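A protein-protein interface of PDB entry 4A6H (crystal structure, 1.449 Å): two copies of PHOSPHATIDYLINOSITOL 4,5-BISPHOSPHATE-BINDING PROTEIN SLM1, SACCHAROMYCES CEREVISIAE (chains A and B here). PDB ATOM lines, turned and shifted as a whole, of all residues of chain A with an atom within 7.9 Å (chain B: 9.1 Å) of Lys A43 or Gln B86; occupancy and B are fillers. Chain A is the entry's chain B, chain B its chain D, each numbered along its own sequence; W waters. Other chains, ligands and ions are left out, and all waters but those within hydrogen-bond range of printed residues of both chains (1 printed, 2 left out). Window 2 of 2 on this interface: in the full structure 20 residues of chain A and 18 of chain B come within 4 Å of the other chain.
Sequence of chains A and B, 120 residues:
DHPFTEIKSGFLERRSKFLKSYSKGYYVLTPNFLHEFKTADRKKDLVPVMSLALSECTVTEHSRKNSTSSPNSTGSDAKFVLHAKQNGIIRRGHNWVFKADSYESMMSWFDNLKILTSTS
OG of Ser B55 lies within hydrogen-bond range of ND1 of His A2. The backbone carbonyl oxygen (O) of Lys A43 sits close to the side-chain amide oxygen (OE1) of Gln B86 (2.9 Å). O of Lys A44 lies close to OE2 of Glu B56 (3.4 Å).
OD1 of Asp A41 lies close to N of Lys A43, at 3.2 Å. The backbone NH (N) of Lys A44 is in hydrogen-bond range of the side-chain carboxylate (OD1) of Asp A41, 3.2 Å away. O of Ala B53 sits at hydrogen-bond distance from SG of Cys B57. The backbone carbonyl oxygen (O) of Ser B55 sits at hydrogen-bond distance from the side-chain amino group (NZ) of Lys B85 (3.4 Å). N of Lys B85 is in hydrogen-bond range of O of Glu B56, 2.8 Å away. The side-chain carboxylate of Glu B56 sits close to the side-chain amide oxygen of Gln B86 (3.4 Å).
His A2 touches Gln B86 (CE1 to NE2, 3.1 Å). CB of Leu A46 touches CB of Ala B53, 3.5 Å away. Leu A46 touches Ser B55 (CD2 to OG, 3.1 Å). Leu A46 touches Glu B56.
Lys A43 touches just one residue of chain B: Gln B86. Of the printed residues of chain B, Lys A44 touches Glu B56 (3.4 Å). Printed residues of chain B within 4 Å of Leu A46: Ala B53 (3.5 Å), Ser B55 (3.1 Å) and Glu B56 (3.0 Å). Ala B84 touches none of the printed residues of chain A. Of chain A, only His A2 (3.1 Å) and Lys A43 (2.9 Å) come within 4 Å of Gln B86.
Hydrophobic or aromatic side chains of chain A that line the printed part of chain B: His A2 and Leu A46. Of the 19 printed residues of chain B, 4 touch a printed residue of chain A. Printed residues of chain B that touch a printed residue of chain A: Ala B53, Ser B55, Glu B56 and Gln B86. Along chain B the printed residues that touch a printed residue of chain A span positions 53 to 86. Among the printed residues, no Asp or Glu carboxylate lies within 4 Å of a Lys or Arg side-chain nitrogen of the other chain.
No position is printed for both chains. Of the 7 pairs that touch across the chains among the printed residues, none has its exchanged pair printed and touching as well.
Water W1 lies within hydrogen-bond range of the backbone carbonyl oxygen of Leu A46 and the backbone NH of Ala B53.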
ATOM      1  N   HIS A   2      -8.940  13.992   2.952  1.00  0.00           N
ATOM      2  CA  HIS A   2     -10.289  14.542   2.854  1.00  0.00           C
ATOM      3  C   HIS A   2     -10.381  15.684   1.840  1.00  0.00           C
ATOM      4  O   HIS A   2     -10.649  16.826   2.218  1.00  0.00           O
ATOM      5  CB  HIS A   2     -10.766  15.038   4.228  1.00  0.00           C
ATOM      6  CG  HIS A   2     -10.788  13.977   5.283  1.00  0.00           C
ATOM      7  ND1 HIS A   2     -11.897  13.196   5.535  1.00  0.00           N
ATOM      8  CD2 HIS A   2      -9.835  13.567   6.154  1.00  0.00           C
ATOM      9  CE1 HIS A   2     -11.624  12.348   6.509  1.00  0.00           C
ATOM     10  NE2 HIS A   2     -10.379  12.551   6.902  1.00  0.00           N
ATOM     11  N   THR A  39     -19.172  23.171  12.918  1.00  0.00           N
ATOM     12  CA  THR A  39     -17.771  23.469  13.204  1.00  0.00           C
ATOM     13  C   THR A  39     -16.904  23.391  11.957  1.00  0.00           C
ATOM     14  O   THR A  39     -17.356  22.950  10.882  1.00  0.00           O
ATOM     15  CB  THR A  39     -17.153  22.477  14.214  1.00  0.00           C
ATOM     16  OG1 THR A  39     -16.928  21.216  13.565  1.00  0.00           O
ATOM     17  CG2 THR A  39     -18.049  22.273  15.434  1.00  0.00           C
ATOM     18  N   ALA A  40     -15.644  23.795  12.111  1.00  0.00           N
ATOM     19  CA  ALA A  40     -14.687  23.793  11.017  1.00  0.00           C
ATOM     20  C   ALA A  40     -13.881  22.511  10.919  1.00  0.00           C
ATOM     21  O   ALA A  40     -12.905  22.460  10.175  1.00  0.00           O
ATOM     22  CB  ALA A  40     -13.743  24.986  11.127  1.00  0.00           C
ATOM     23  N   ASP A  41     -14.277  21.472  11.644  1.00  0.00           N
ATOM     24  CA  ASP A  41     -13.512  20.224  11.606  1.00  0.00           C
ATOM     25  C   ASP A  41     -13.797  19.498  10.288  1.00  0.00           C
ATOM     26  O   ASP A  41     -14.714  18.690  10.195  1.00  0.00           O
ATOM     27  CB  ASP A  41     -13.777  19.371  12.847  1.00  0.00           C
ATOM     28  CG  ASP A  41     -12.877  18.158  12.911  1.00  0.00           C
ATOM     29  OD1 ASP A  41     -12.236  17.852  11.880  1.00  0.00           O
ATOM     30  OD2 ASP A  41     -12.782  17.550  13.992  1.00  0.00           O
ATOM     31  N   ARG A  42     -12.991  19.814   9.282  1.00  0.00           N
ATOM     32  CA  ARG A  42     -13.231  19.376   7.910  1.00  0.00           C
ATOM     33  C   ARG A  42     -12.920  17.898   7.714  1.00  0.00           C
ATOM     34  O   ARG A  42     -13.184  17.340   6.646  1.00  0.00           O
ATOM     35  CB  ARG A  42     -12.416  20.229   6.934  1.00  0.00           C
ATOM     36  CG  ARG A  42     -12.670  21.732   7.077  1.00  0.00           C
ATOM     37  CD  ARG A  42     -14.128  22.074   6.796  1.00  0.00           C
ATOM     38  NE  ARG A  42     -14.516  21.622   5.465  1.00  0.00           N
ATOM     39  CZ  ARG A  42     -15.595  20.894   5.192  1.00  0.00           C
ATOM     40  NH1 ARG A  42     -16.427  20.540   6.161  1.00  0.00           N
ATOM     41  NH2 ARG A  42     -15.842  20.526   3.939  1.00  0.00           N
ATOM     42  N   LYS A  43     -12.364  17.265   8.742  1.00  0.00           N
ATOM     43  CA  LYS A  43     -12.062  15.839   8.677  1.00  0.00           C
ATOM     44  C   LYS A  43     -13.123  14.986   9.355  1.00  0.00           C
ATOM     45  O   LYS A  43     -13.271  13.813   9.021  1.00  0.00           O
ATOM     46  CB  LYS A  43     -10.699  15.536   9.308  1.00  0.00           C
ATOM     47  CG  LYS A  43      -9.649  16.607   9.073  1.00  0.00           C
ATOM     48  CD  LYS A  43      -8.479  16.070   8.271  1.00  0.00           C
ATOM     49  CE  LYS A  43      -7.336  17.074   8.232  1.00  0.00           C
ATOM     50  NZ  LYS A  43      -6.230  16.616   7.344  1.00  0.00           N
ATOM     51  N   LYS A  44     -13.868  15.563  10.295  1.00  0.00           N
ATOM     52  CA  LYS A  44     -14.825  14.782  11.087  1.00  0.00           C
ATOM     53  C   LYS A  44     -16.276  15.296  11.097  1.00  0.00           C
ATOM     54  O   LYS A  44     -17.211  14.502  11.203  1.00  0.00           O
ATOM     55  CB  LYS A  44     -14.325  14.591  12.521  1.00  0.00           C
ATOM     56  CG  LYS A  44     -13.054  13.758  12.621  1.00  0.00           C
ATOM     57  CD  LYS A  44     -12.646  13.533  14.069  1.00  0.00           C
ATOM     58  CE  LYS A  44     -13.719  12.790  14.842  1.00  0.00           C
ATOM     59  NZ  LYS A  44     -13.291  12.510  16.241  1.00  0.00           N
ATOM     60  N   ASP A  45     -16.468  16.608  10.986  1.00  0.00           N
ATOM     61  CA  ASP A  45     -17.813  17.196  11.033  1.00  0.00           C
ATOM     62  C   ASP A  45     -18.320  17.416   9.606  1.00  0.00           C
ATOM     63  O   ASP A  45     -18.171  18.495   9.047  1.00  0.00           O
ATOM     64  CB  ASP A  45     -17.777  18.516  11.825  1.00  0.00           C
ATOM     65  CG  ASP A  45     -19.135  19.213  11.903  1.00  0.00           C
ATOM     66  OD1 ASP A  45     -20.166  18.622  11.513  1.00  0.00           O
ATOM     67  OD2 ASP A  45     -19.163  20.381  12.349  1.00  0.00           O
ATOM     68  N   LEU A  46     -18.872  16.358   9.016  1.00  0.00           N
ATOM     69  CA  LEU A  46     -19.198  16.377   7.593  1.00  0.00           C
ATOM     70  C   LEU A  46     -20.671  16.099   7.262  1.00  0.00           C
ATOM     71  O   LEU A  46     -20.994  15.804   6.114  1.00  0.00           O
ATOM     72  CB  LEU A  46     -18.286  15.422   6.805  1.00  0.00           C
ATOM     73  CG  LEU A  46     -16.768  15.622   6.855  1.00  0.00           C
ATOM     74  CD1 LEU A  46     -16.187  14.802   7.980  1.00  0.00           C
ATOM     75  CD2 LEU A  46     -16.113  15.220   5.547  1.00  0.00           C
ATOM     76  N   LEU B  52     -24.179  12.264   2.166  1.00  0.00           N
ATOM     77  CA  LEU B  52     -23.164  11.351   2.703  1.00  0.00           C
ATOM     78  C   LEU B  52     -21.787  11.796   2.233  1.00  0.00           C
ATOM     79  O   LEU B  52     -21.492  11.757   1.043  1.00  0.00           O
ATOM     80  CB  LEU B  52     -23.426   9.929   2.194  1.00  0.00           C
ATOM     81  CG  LEU B  52     -24.691   9.201   2.655  1.00  0.00           C
ATOM     82  CD1 LEU B  52     -25.043   8.053   1.703  1.00  0.00           C
ATOM     83  CD2 LEU B  52     -24.509   8.673   4.063  1.00  0.00           C
ATOM     84  N   ALA B  53     -20.940  12.218   3.167  1.00  0.00           N
ATOM     85  CA  ALA B  53     -19.610  12.701   2.808  1.00  0.00           C
ATOM     86  C   ALA B  53     -18.701  11.568   2.339  1.00  0.00           C
ATOM     87  O   ALA B  53     -18.389  10.656   3.100  1.00  0.00           O
ATOM     88  CB  ALA B  53     -18.971  13.433   3.997  1.00  0.00           C
ATOM     89  N   LEU B  54     -18.266  11.650   1.090  1.00  0.00           N
ATOM     90  CA  LEU B  54     -17.437  10.607   0.489  1.00  0.00           C
ATOM     91  C   LEU B  54     -16.101  10.384   1.198  1.00  0.00           C
ATOM     92  O   LEU B  54     -15.592   9.266   1.213  1.00  0.00           O
ATOM     93  CB  LEU B  54     -17.196  10.906  -0.987  1.00  0.00           C
ATOM     94  CG  LEU B  54     -18.442  11.060  -1.860  1.00  0.00           C
ATOM     95  CD1 LEU B  54     -18.045  11.321  -3.299  1.00  0.00           C
ATOM     96  CD2 LEU B  54     -19.308   9.816  -1.765  1.00  0.00           C
ATOM     97  N   SER B  55     -15.531  11.439   1.767  1.00  0.00           N
ATOM     98  CA  SER B  55     -14.236  11.304   2.437  1.00  0.00           C
ATOM     99  C   SER B  55     -14.307  10.439   3.695  1.00  0.00           C
ATOM    100  O   SER B  55     -13.271  10.046   4.240  1.00  0.00           O
ATOM    101  CB  SER B  55     -13.666  12.674   2.787  1.00  0.00           C
ATOM    102  OG  SER B  55     -14.411  13.261   3.835  1.00  0.00           O
ATOM    103  N   GLU B  56     -15.524  10.167   4.156  1.00  0.00           N
ATOM    104  CA  GLU B  56     -15.770   9.320   5.316  1.00  0.00           C
ATOM    105  C   GLU B  56     -16.229   7.914   4.930  1.00  0.00           C
ATOM    106  O   GLU B  56     -16.572   7.127   5.809  1.00  0.00           O
ATOM    107  CB  GLU B  56     -16.864   9.938   6.195  1.00  0.00           C
ATOM    108  CG  GLU B  56     -16.557  11.323   6.746  1.00  0.00           C
ATOM    109  CD  GLU B  56     -17.660  11.835   7.660  1.00  0.00           C
ATOM    110  OE1 GLU B  56     -18.821  11.929   7.210  1.00  0.00           O
ATOM    111  OE2 GLU B  56     -17.367  12.134   8.836  1.00  0.00           O
ATOM    112  N   CYS B  57     -16.247   7.607   3.632  1.00  0.00           N
ATOM    113  CA  CYS B  57     -16.785   6.327   3.147  1.00  0.00           C
ATOM    114  C   CYS B  57     -15.788   5.565   2.281  1.00  0.00           C
ATOM    115  O   CYS B  57     -14.806   6.135   1.803  1.00  0.00           O
ATOM    116  CB  CYS B  57     -18.066   6.545   2.330  1.00  0.00           C
ATOM    117  SG  CYS B  57     -19.425   7.325   3.215  1.00  0.00           S
ATOM    118  N   THR B  58     -16.054   4.276   2.085  1.00  0.00           N
ATOM    119  CA  THR B  58     -15.367   3.495   1.068  1.00  0.00           C
ATOM    120  C   THR B  58     -16.420   2.619   0.406  1.00  0.00           C
ATOM    121  O   THR B  58     -17.469   2.377   0.994  1.00  0.00           O
ATOM    122  CB  THR B  58     -14.267   2.617   1.675  1.00  0.00           C
ATOM    123  OG1 THR B  58     -14.837   1.757   2.663  1.00  0.00           O
ATOM    124  CG2 THR B  58     -13.195   3.475   2.332  1.00  0.00           C
ATOM    125  N   HIS B  83     -19.309   1.582   2.799  1.00  0.00           N
ATOM    126  CA  HIS B  83     -18.850   1.372   4.161  1.00  0.00           C
ATOM    127  C   HIS B  83     -18.495   2.693   4.830  1.00  0.00           C
ATOM    128  O   HIS B  83     -17.832   3.526   4.228  1.00  0.00           O
ATOM    129  CB  HIS B  83     -17.623   0.456   4.146  1.00  0.00           C
ATOM    130  CG  HIS B  83     -16.982   0.282   5.488  1.00  0.00           C
ATOM    131  ND1 HIS B  83     -17.449  -0.615   6.422  1.00  0.00           N
ATOM    132  CD2 HIS B  83     -15.913   0.890   6.051  1.00  0.00           C
ATOM    133  CE1 HIS B  83     -16.697  -0.550   7.506  1.00  0.00           C
ATOM    134  NE2 HIS B  83     -15.756   0.354   7.305  1.00  0.00           N
ATOM    135  N   ALA B  84     -18.914   2.877   6.081  1.00  0.00           N
ATOM    136  CA  ALA B  84     -18.584   4.104   6.810  1.00  0.00           C
ATOM    137  C   ALA B  84     -17.285   3.945   7.599  1.00  0.00           C
ATOM    138  O   ALA B  84     -17.171   3.074   8.458  1.00  0.00           O
ATOM    139  CB  ALA B  84     -19.720   4.505   7.737  1.00  0.00           C
ATOM    140  N   LYS B  85     -16.307   4.795   7.306  1.00  0.00           N
ATOM    141  CA  LYS B  85     -15.043   4.809   8.039  1.00  0.00           C
ATOM    142  C   LYS B  85     -15.132   5.656   9.309  1.00  0.00           C
ATOM    143  O   LYS B  85     -14.312   5.501  10.223  1.00  0.00           O
ATOM    144  CB  LYS B  85     -13.913   5.342   7.156  1.00  0.00           C
ATOM    145  CG  LYS B  85     -13.635   4.518   5.917  1.00  0.00           C
ATOM    146  CD  LYS B  85     -12.449   5.079   5.152  1.00  0.00           C
ATOM    147  CE  LYS B  85     -12.704   6.512   4.716  1.00  0.00           C
ATOM    148  NZ  LYS B  85     -11.581   7.069   3.907  1.00  0.00           N
ATOM    149  N   GLN B  86     -16.123   6.546   9.362  1.00  0.00           N
ATOM    150  CA  GLN B  86     -16.302   7.465  10.483  1.00  0.00           C
ATOM    151  C   GLN B  86     -17.784   7.698  10.762  1.00  0.00           C
ATOM    152  O   GLN B  86     -18.627   7.463   9.895  1.00  0.00           O
ATOM    153  CB  GLN B  86     -15.638   8.810  10.172  1.00  0.00           C
ATOM    154  CG  GLN B  86     -14.272   8.702   9.510  1.00  0.00           C
ATOM    155  CD  GLN B  86     -13.832  10.009   8.876  1.00  0.00           C
ATOM    156  OE1 GLN B  86     -14.190  11.092   9.344  1.00  0.00           O
ATOM    157  NE2 GLN B  86     -13.055   9.915   7.801  1.00  0.00           N
ATOM    158  N   ASN B  87     -18.099   8.170  11.965  1.00  0.00           N
ATOM    159  CA  ASN B  87     -19.475   8.490  12.329  1.00  0.00           C
ATOM    160  C   ASN B  87     -19.997   9.712  11.575  1.00  0.00           C
ATOM    161  O   ASN B  87     -19.358  10.762  11.566  1.00  0.00           O
ATOM    162  CB  ASN B  87     -19.598   8.740  13.835  1.00  0.00           C
ATOM    163  CG  ASN B  87     -19.428   7.478  14.654  1.00  0.00           C
ATOM    164  OD1 ASN B  87     -20.187   6.521  14.508  1.00  0.00           O
ATOM    165  ND2 ASN B  87     -18.435   7.475  15.535  1.00  0.00           N
ATOM    166  N   GLY B  88     -21.158   9.567  10.946  1.00  0.00           N
ATOM    167  CA  GLY B  88     -21.791  10.670  10.245  1.00  0.00           C
ATOM    168  C   GLY B  88     -23.265  10.369  10.118  1.00  0.00           C
ATOM    169  O   GLY B  88     -23.992  10.322  11.111  1.00  0.00           O
ATOM    170  N   ILE B  89     -23.712  10.157   8.889  1.00  0.00           N
ATOM    171  CA  ILE B  89     -25.057   9.654   8.665  1.00  0.00           C
ATOM    172  C   ILE B  89     -25.104   8.183   9.057  1.00  0.00           C
ATOM    173  O   ILE B  89     -26.103   7.693   9.585  1.00  0.00           O
ATOM    174  CB  ILE B  89     -25.453   9.764   7.188  1.00  0.00           C
ATOM    175  CG1 ILE B  89     -25.423  11.223   6.718  1.00  0.00           C
ATOM    176  CG2 ILE B  89     -26.822   9.137   6.974  1.00  0.00           C
ATOM    177  CD1 ILE B  89     -26.518  12.077   7.309  1.00  0.00           C
ATOM    178  N   ILE B  90     -24.013   7.484   8.768  1.00  0.00           N
ATOM    179  CA  ILE B  90     -23.871   6.071   9.083  1.00  0.00           C
ATOM    180  C   ILE B  90     -22.912   5.948  10.264  1.00  0.00           C
ATOM    181  O   ILE B  90     -21.935   6.693  10.352  1.00  0.00           O
ATOM    182  CB  ILE B  90     -23.299   5.303   7.873  1.00  0.00           C
ATOM    183  CG1 ILE B  90     -24.160   5.551   6.628  1.00  0.00           C
ATOM    184  CG2 ILE B  90     -23.192   3.809   8.181  1.00  0.00           C
ATOM    185  CD1 ILE B  90     -23.556   5.006   5.346  1.00  0.00           C
ATOM    186  N   ARG B  91     -23.188   5.031  11.186  1.00  0.00           N
ATOM    187  CA  ARG B  91     -22.273   4.833  12.307  1.00  0.00           C
ATOM    188  C   ARG B  91     -20.962   4.226  11.812  1.00  0.00           C
ATOM    189  O   ARG B  91     -20.961   3.392  10.909  1.00  0.00           O
ATOM    190  CB  ARG B  91     -22.898   3.944  13.387  1.00  0.00           C
ATOM    191  CG  ARG B  91     -24.115   4.546  14.070  1.00  0.00           C
ATOM    192  N   ARG B  92     -19.846   4.646  12.401  1.00  0.00           N
ATOM    193  CA  ARG B  92     -18.541   4.127  12.011  1.00  0.00           C
ATOM    194  C   ARG B  92     -18.502   2.594  11.988  1.00  0.00           C
ATOM    195  O   ARG B  92     -18.922   1.935  12.943  1.00  0.00           O
ATOM    196  CB  ARG B  92     -17.457   4.644  12.965  1.00  0.00           C
ATOM    197  CG  ARG B  92     -16.073   4.100  12.673  1.00  0.00           C
ATOM    198  CD  ARG B  92     -15.022   4.719  13.589  1.00  0.00           C
ATOM    199  NE  ARG B  92     -15.350   4.543  15.000  1.00  0.00           N
ATOM    200  N   GLY B  93     -17.978   2.036  10.899  1.00  0.00           N
ATOM    201  CA  GLY B  93     -17.815   0.601  10.760  1.00  0.00           C
ATOM    202  C   GLY B  93     -19.012  -0.110  10.159  1.00  0.00           C
ATOM    203  O   GLY B  93     -18.936  -1.297   9.832  1.00  0.00           O
ATOM    204  N   HIS B  94     -20.125   0.608  10.029  1.00  0.00           N
ATOM    205  CA  HIS B  94     -21.342   0.031   9.471  1.00  0.00           C
ATOM    206  C   HIS B  94     -21.405   0.163   7.943  1.00  0.00           C
ATOM    207  O   HIS B  94     -20.590   0.858   7.338  1.00  0.00           O
ATOM    208  CB  HIS B  94     -22.576   0.651  10.132  1.00  0.00           C
ATOM    209  CG  HIS B  94     -22.805   0.182  11.534  1.00  0.00           C
ATOM    210  ND1 HIS B  94     -21.881   0.365  12.540  1.00  0.00           N
ATOM    211  CD2 HIS B  94     -23.851  -0.467  12.097  1.00  0.00           C
ATOM    212  CE1 HIS B  94     -22.346  -0.151  13.663  1.00  0.00           C
ATOM    213  NE2 HIS B  94     -23.541  -0.662  13.422  1.00  0.00           N
HETATM  214  O   HOH W   1     -22.205  13.239   5.690  1.00  0.00           O
